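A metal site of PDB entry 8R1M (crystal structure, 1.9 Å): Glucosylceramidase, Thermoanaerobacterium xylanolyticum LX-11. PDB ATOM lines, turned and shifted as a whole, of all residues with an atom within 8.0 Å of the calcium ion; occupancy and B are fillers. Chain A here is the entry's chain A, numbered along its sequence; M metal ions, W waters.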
ATOM      1  N   LEU A 556      22.988  12.664 -14.854  1.00  0.00           N
ATOM      2  CA  LEU A 556      22.824  13.799 -13.968  1.00  0.00           C
ATOM      3  C   LEU A 556      24.197  14.421 -13.680  1.00  0.00           C
ATOM      4  O   LEU A 556      24.330  15.647 -13.614  1.00  0.00           O
ATOM      5  CB  LEU A 556      22.125  13.281 -12.712  1.00  0.00           C
ATOM      6  CG  LEU A 556      21.180  14.250 -11.987  1.00  0.00           C
ATOM      7  CD1 LEU A 556      20.227  14.989 -12.890  1.00  0.00           C
ATOM      8  CD2 LEU A 556      20.416  13.474 -10.920  1.00  0.00           C
ATOM      9  N   LYS A 557      25.238  13.591 -13.566  1.00  0.00           N
ATOM     10  CA  LYS A 557      26.570  14.108 -13.289  1.00  0.00           C
ATOM     11  C   LYS A 557      26.992  15.114 -14.371  1.00  0.00           C
ATOM     12  O   LYS A 557      27.643  16.103 -14.074  1.00  0.00           O
ATOM     13  CB  LYS A 557      27.605  12.992 -13.184  1.00  0.00           C
ATOM     14  CG  LYS A 557      29.029  13.453 -12.866  1.00  0.00           C
ATOM     15  CD  LYS A 557      29.151  14.297 -11.598  1.00  0.00           C
ATOM     16  CE  LYS A 557      30.429  14.083 -10.864  1.00  0.00           C
ATOM     17  NZ  LYS A 557      31.598  14.255 -11.721  1.00  0.00           N
ATOM     18  N   MET A 559      25.328  17.309 -15.827  1.00  0.00           N
ATOM     19  CA  MET A 559      24.703  18.616 -15.719  1.00  0.00           C
ATOM     20  C   MET A 559      25.383  19.468 -14.641  1.00  0.00           C
ATOM     21  O   MET A 559      24.957  20.584 -14.387  1.00  0.00           O
ATOM     22  CB  MET A 559      23.215  18.486 -15.377  1.00  0.00           C
ATOM     23  CG  MET A 559      22.389  17.877 -16.467  1.00  0.00           C
ATOM     24  SD  MET A 559      20.843  17.212 -15.803  1.00  0.00           S
ATOM     25  CE  MET A 559      19.881  17.249 -17.327  1.00  0.00           C
ATOM     26  N   ASP A 560      26.428  18.913 -14.016  1.00  0.00           N
ATOM     27  CA  ASP A 560      27.310  19.669 -13.129  1.00  0.00           C
ATOM     28  C   ASP A 560      28.218  20.579 -13.959  1.00  0.00           C
ATOM     29  O   ASP A 560      29.368  20.232 -14.185  1.00  0.00           O
ATOM     30  CB  ASP A 560      28.154  18.744 -12.258  1.00  0.00           C
ATOM     31  CG  ASP A 560      29.240  19.397 -11.391  1.00  0.00           C
ATOM     32  OD1 ASP A 560      29.014  20.516 -10.862  1.00  0.00           O
ATOM     33  OD2 ASP A 560      30.290  18.758 -11.170  1.00  0.00           O
ATOM     34  N   LYS A 561      27.716  21.739 -14.377  1.00  0.00           N
ATOM     35  CA  LYS A 561      28.470  22.647 -15.222  1.00  0.00           C
ATOM     36  C   LYS A 561      29.682  23.226 -14.464  1.00  0.00           C
ATOM     37  O   LYS A 561      30.738  23.369 -15.053  1.00  0.00           O
ATOM     38  CB  LYS A 561      27.547  23.711 -15.829  1.00  0.00           C
ATOM     39  N   ASP A 562      29.560  23.507 -13.156  1.00  0.00           N
ATOM     40  CA  ASP A 562      30.589  24.250 -12.454  1.00  0.00           C
ATOM     41  C   ASP A 562      31.559  23.354 -11.680  1.00  0.00           C
ATOM     42  O   ASP A 562      32.337  23.848 -10.871  1.00  0.00           O
ATOM     43  CB  ASP A 562      29.972  25.313 -11.546  1.00  0.00           C
ATOM     44  CG  ASP A 562      29.066  24.791 -10.453  1.00  0.00           C
ATOM     45  OD1 ASP A 562      29.019  23.560 -10.242  1.00  0.00           O
ATOM     46  OD2 ASP A 562      28.364  25.612  -9.846  1.00  0.00           O
ATOM     47  N   ASN A 563      31.527  22.034 -11.904  1.00  0.00           N
ATOM     48  CA  ASN A 563      32.539  21.120 -11.381  1.00  0.00           C
ATOM     49  C   ASN A 563      32.640  21.110  -9.849  1.00  0.00           C
ATOM     50  O   ASN A 563      33.713  20.808  -9.323  1.00  0.00           O
ATOM     51  CB  ASN A 563      33.891  21.374 -12.039  1.00  0.00           C
ATOM     52  CG  ASN A 563      33.784  21.347 -13.538  1.00  0.00           C
ATOM     53  OD1 ASN A 563      33.284  20.377 -14.112  1.00  0.00           O
ATOM     54  ND2 ASN A 563      34.207  22.418 -14.193  1.00  0.00           N
ATOM     55  N   ASP A 564      31.505  21.329  -9.133  1.00  0.00           N
ATOM     56  CA  ASP A 564      31.421  21.113  -7.689  1.00  0.00           C
ATOM     57  C   ASP A 564      30.905  19.711  -7.318  1.00  0.00           C
ATOM     58  O   ASP A 564      30.720  19.423  -6.137  1.00  0.00           O
ATOM     59  CB  ASP A 564      30.553  22.167  -7.003  1.00  0.00           C
ATOM     60  CG  ASP A 564      29.053  22.141  -7.310  1.00  0.00           C
ATOM     61  OD1 ASP A 564      28.606  21.427  -8.266  1.00  0.00           O
ATOM     62  OD2 ASP A 564      28.349  22.889  -6.598  1.00  0.00           O
ATOM     63  N   GLY A 565      30.685  18.857  -8.312  1.00  0.00           N
ATOM     64  CA  GLY A 565      30.282  17.472  -8.086  1.00  0.00           C
ATOM     65  C   GLY A 565      28.758  17.287  -8.019  1.00  0.00           C
ATOM     66  O   GLY A 565      28.317  16.169  -7.742  1.00  0.00           O
ATOM     67  N   ILE A 566      27.993  18.345  -8.301  1.00  0.00           N
ATOM     68  CA  ILE A 566      26.553  18.405  -8.034  1.00  0.00           C
ATOM     69  C   ILE A 566      25.842  18.958  -9.263  1.00  0.00           C
ATOM     70  O   ILE A 566      26.243  20.004  -9.775  1.00  0.00           O
ATOM     71  CB  ILE A 566      26.216  19.305  -6.813  1.00  0.00           C
ATOM     72  CG1 ILE A 566      27.052  18.971  -5.594  1.00  0.00           C
ATOM     73  CG2 ILE A 566      24.712  19.299  -6.489  1.00  0.00           C
ATOM     74  CD1 ILE A 566      26.774  19.859  -4.385  1.00  0.00           C
ATOM     75  N   PRO A 567      24.734  18.361  -9.742  1.00  0.00           N
ATOM     76  CA  PRO A 567      24.007  18.925 -10.872  1.00  0.00           C
ATOM     77  C   PRO A 567      23.691  20.382 -10.565  1.00  0.00           C
ATOM     78  O   PRO A 567      23.395  20.725  -9.426  1.00  0.00           O
ATOM     79  CB  PRO A 567      22.753  18.067 -11.006  1.00  0.00           C
ATOM     80  CG  PRO A 567      23.087  16.794 -10.253  1.00  0.00           C
ATOM     81  CD  PRO A 567      24.114  17.135  -9.210  1.00  0.00           C
ATOM     82  N   ASP A 568      23.768  21.235 -11.593  1.00  0.00           N
ATOM     83  CA  ASP A 568      23.450  22.649 -11.445  1.00  0.00           C
ATOM     84  C   ASP A 568      21.994  22.904 -11.834  1.00  0.00           C
ATOM     85  O   ASP A 568      21.621  22.633 -12.954  1.00  0.00           O
ATOM     86  CB  ASP A 568      24.331  23.531 -12.302  1.00  0.00           C
ATOM     87  CG  ASP A 568      25.842  23.414 -12.096  1.00  0.00           C
ATOM     88  OD1 ASP A 568      26.313  22.478 -11.392  1.00  0.00           O
ATOM     89  OD2 ASP A 568      26.546  24.251 -12.683  1.00  0.00           O
ATOM     90  N   ASN A 569      21.196  23.463 -10.903  1.00  0.00           N
ATOM     91  CA  ASN A 569      19.934  24.080 -11.275  1.00  0.00           C
ATOM     92  C   ASN A 569      20.242  25.265 -12.195  1.00  0.00           C
ATOM     93  O   ASN A 569      21.245  25.931 -12.008  1.00  0.00           O
ATOM     94  CB  ASN A 569      19.095  24.456 -10.049  1.00  0.00           C
ATOM     95  CG  ASN A 569      18.593  23.233  -9.310  1.00  0.00           C
ATOM     96  OD1 ASN A 569      19.130  22.853  -8.268  1.00  0.00           O
ATOM     97  ND2 ASN A 569      17.610  22.554  -9.878  1.00  0.00           N
ATOM     98  N   GLY A 584      22.017  27.044  -9.477  1.00  0.00           N
ATOM     99  CA  GLY A 584      23.255  26.636  -8.849  1.00  0.00           C
ATOM    100  C   GLY A 584      23.041  25.327  -8.104  1.00  0.00           C
ATOM    101  O   GLY A 584      22.346  24.444  -8.587  1.00  0.00           O
ATOM    102  N   THR A 585      23.670  25.193  -6.952  1.00  0.00           N
ATOM    103  CA  THR A 585      23.364  24.075  -6.088  1.00  0.00           C
ATOM    104  C   THR A 585      22.177  24.479  -5.233  1.00  0.00           C
ATOM    105  O   THR A 585      22.190  25.565  -4.650  1.00  0.00           O
ATOM    106  CB  THR A 585      24.575  23.720  -5.242  1.00  0.00           C
ATOM    107  OG1 THR A 585      25.584  23.295  -6.159  1.00  0.00           O
ATOM    108  CG2 THR A 585      24.279  22.587  -4.276  1.00  0.00           C
ATOM    109  N   TRP A 593      20.434  14.306  -4.671  1.00  0.00           N
ATOM    110  CA  TRP A 593      21.604  13.796  -5.357  1.00  0.00           C
ATOM    111  C   TRP A 593      22.539  13.065  -4.404  1.00  0.00           C
ATOM    112  O   TRP A 593      23.008  11.966  -4.711  1.00  0.00           O
ATOM    113  CB  TRP A 593      22.290  14.964  -6.068  1.00  0.00           C
ATOM    114  CG  TRP A 593      23.656  14.711  -6.639  1.00  0.00           C
ATOM    115  CD1 TRP A 593      24.819  15.291  -6.231  1.00  0.00           C
ATOM    116  CD2 TRP A 593      23.997  13.879  -7.765  1.00  0.00           C
ATOM    117  NE1 TRP A 593      25.867  14.841  -6.987  1.00  0.00           N
ATOM    118  CE2 TRP A 593      25.394  13.998  -7.953  1.00  0.00           C
ATOM    119  CE3 TRP A 593      23.264  13.045  -8.621  1.00  0.00           C
ATOM    120  CZ2 TRP A 593      26.073  13.314  -8.960  1.00  0.00           C
ATOM    121  CZ3 TRP A 593      23.936  12.373  -9.619  1.00  0.00           C
ATOM    122  CH2 TRP A 593      25.328  12.524  -9.799  1.00  0.00           C
ATOM    123  N   ASN A 626      31.037  19.792  -0.727  1.00  0.00           N
ATOM    124  CA  ASN A 626      30.712  21.005  -1.446  1.00  0.00           C
ATOM    125  C   ASN A 626      29.300  21.455  -1.079  1.00  0.00           C
ATOM    126  O   ASN A 626      29.058  22.633  -0.885  1.00  0.00           O
ATOM    127  CB  ASN A 626      30.976  20.844  -2.939  1.00  0.00           C
ATOM    128  CG  ASN A 626      32.449  20.693  -3.250  1.00  0.00           C
ATOM    129  OD1 ASN A 626      33.307  20.920  -2.384  1.00  0.00           O
ATOM    130  ND2 ASN A 626      32.773  20.297  -4.467  1.00  0.00           N
ATOM    131  N   GLU A 630      28.643  25.010   0.592  1.00  0.00           N
ATOM    132  CA  GLU A 630      27.949  25.969  -0.247  1.00  0.00           C
ATOM    133  C   GLU A 630      26.655  26.469   0.394  1.00  0.00           C
ATOM    134  O   GLU A 630      26.214  27.572   0.069  1.00  0.00           O
ATOM    135  CB  GLU A 630      27.644  25.396  -1.639  1.00  0.00           C
ATOM    136  CG  GLU A 630      28.852  25.208  -2.560  1.00  0.00           C
ATOM    137  CD  GLU A 630      28.489  24.491  -3.860  1.00  0.00           C
ATOM    138  OE1 GLU A 630      27.292  24.402  -4.203  1.00  0.00           O
ATOM    139  OE2 GLU A 630      29.420  24.009  -4.530  1.00  0.00           O
ATOM    140  N   THR A 641      22.355  28.418  -4.362  1.00  0.00           N
ATOM    141  CA  THR A 641      23.565  29.217  -4.303  1.00  0.00           C
ATOM    142  C   THR A 641      23.423  30.534  -5.066  1.00  0.00           C
ATOM    143  O   THR A 641      24.219  31.438  -4.839  1.00  0.00           O
ATOM    144  CB  THR A 641      24.787  28.436  -4.800  1.00  0.00           C
ATOM    145  OG1 THR A 641      24.467  27.827  -6.049  1.00  0.00           O
ATOM    146  CG2 THR A 641      25.276  27.408  -3.799  1.00  0.00           C
ATOM    147  N   GLU A 642      22.448  30.696  -5.956  1.00  0.00           N
ATOM    148  CA  GLU A 642      22.564  31.792  -6.923  1.00  0.00           C
ATOM    149  C   GLU A 642      21.273  32.558  -7.164  1.00  0.00           C
ATOM    150  O   GLU A 642      21.314  33.512  -7.928  1.00  0.00           O
ATOM    151  CB  GLU A 642      23.120  31.289  -8.260  1.00  0.00           C
ATOM    152  CG  GLU A 642      24.559  30.776  -8.203  1.00  0.00           C
ATOM    153  CD  GLU A 642      25.079  30.191  -9.503  1.00  0.00           C
ATOM    154  OE1 GLU A 642      24.519  30.513 -10.570  1.00  0.00           O
ATOM    155  OE2 GLU A 642      26.031  29.383  -9.468  1.00  0.00           O
HETATM  156 CA    CA M   1      27.468  21.871  -9.873  1.00  0.00          CA
HETATM  157  O   HOH W   1      25.642  23.054  -8.902  1.00  0.00           O
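The side-chain carboxylate of Asp 568 is in hydrogen-bond range of the backbone NH of Lys 561, 3.2 Å away. The backbone NH (N) of Asp 568 lies within hydrogen-bond range of the backbone carbonyl oxygen (O) of Met 559 (3.1 Å). The side-chain hydroxyl (OG1) of Thr 585 is in hydrogen-bond range of the side-chain carboxylate (OD2) of Asp 564, 2.8 Å away. OE2 of Glu 630 sits close to OD2 of Asp 564 (2.6 Å). O of Asp 564 sits at hydrogen-bond distance from ND2 of Asn 626, 2.8 Å away. OD1 of Asp 560 lies close to N of Asn 563, at 3.1 Å. The side-chain carboxylate of Asp 560 lies within hydrogen-bond range of the backbone NH of Gly 565 (2.9 Å).
Within 4 Å of the calcium ion: Asp 560, Asp 562, Asp 564, Ile 566 and Asp 568. The nearest printed residue that does not touch the calcium ion is Pro 567 (4.1 Å).
The calcium ion is bound by OD1 of Asp 568 (2.0 Å). OD1 of Asp 564 is bound to the calcium ion (2.0 Å). The calcium ion is bound by O of Ile 566, at 2.2 Å. The calcium ion is bound by the side-chain carboxylate (OD1) of Asp 560 (2.3 Å). OD1 of Asp 562 binds the calcium ion (2.3 Å). Water W1 is bound to the calcium ion.
Water W1 bridges OG1 of Thr 585 (2.8 Å) and O of Pro 567 (3.3 Å).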
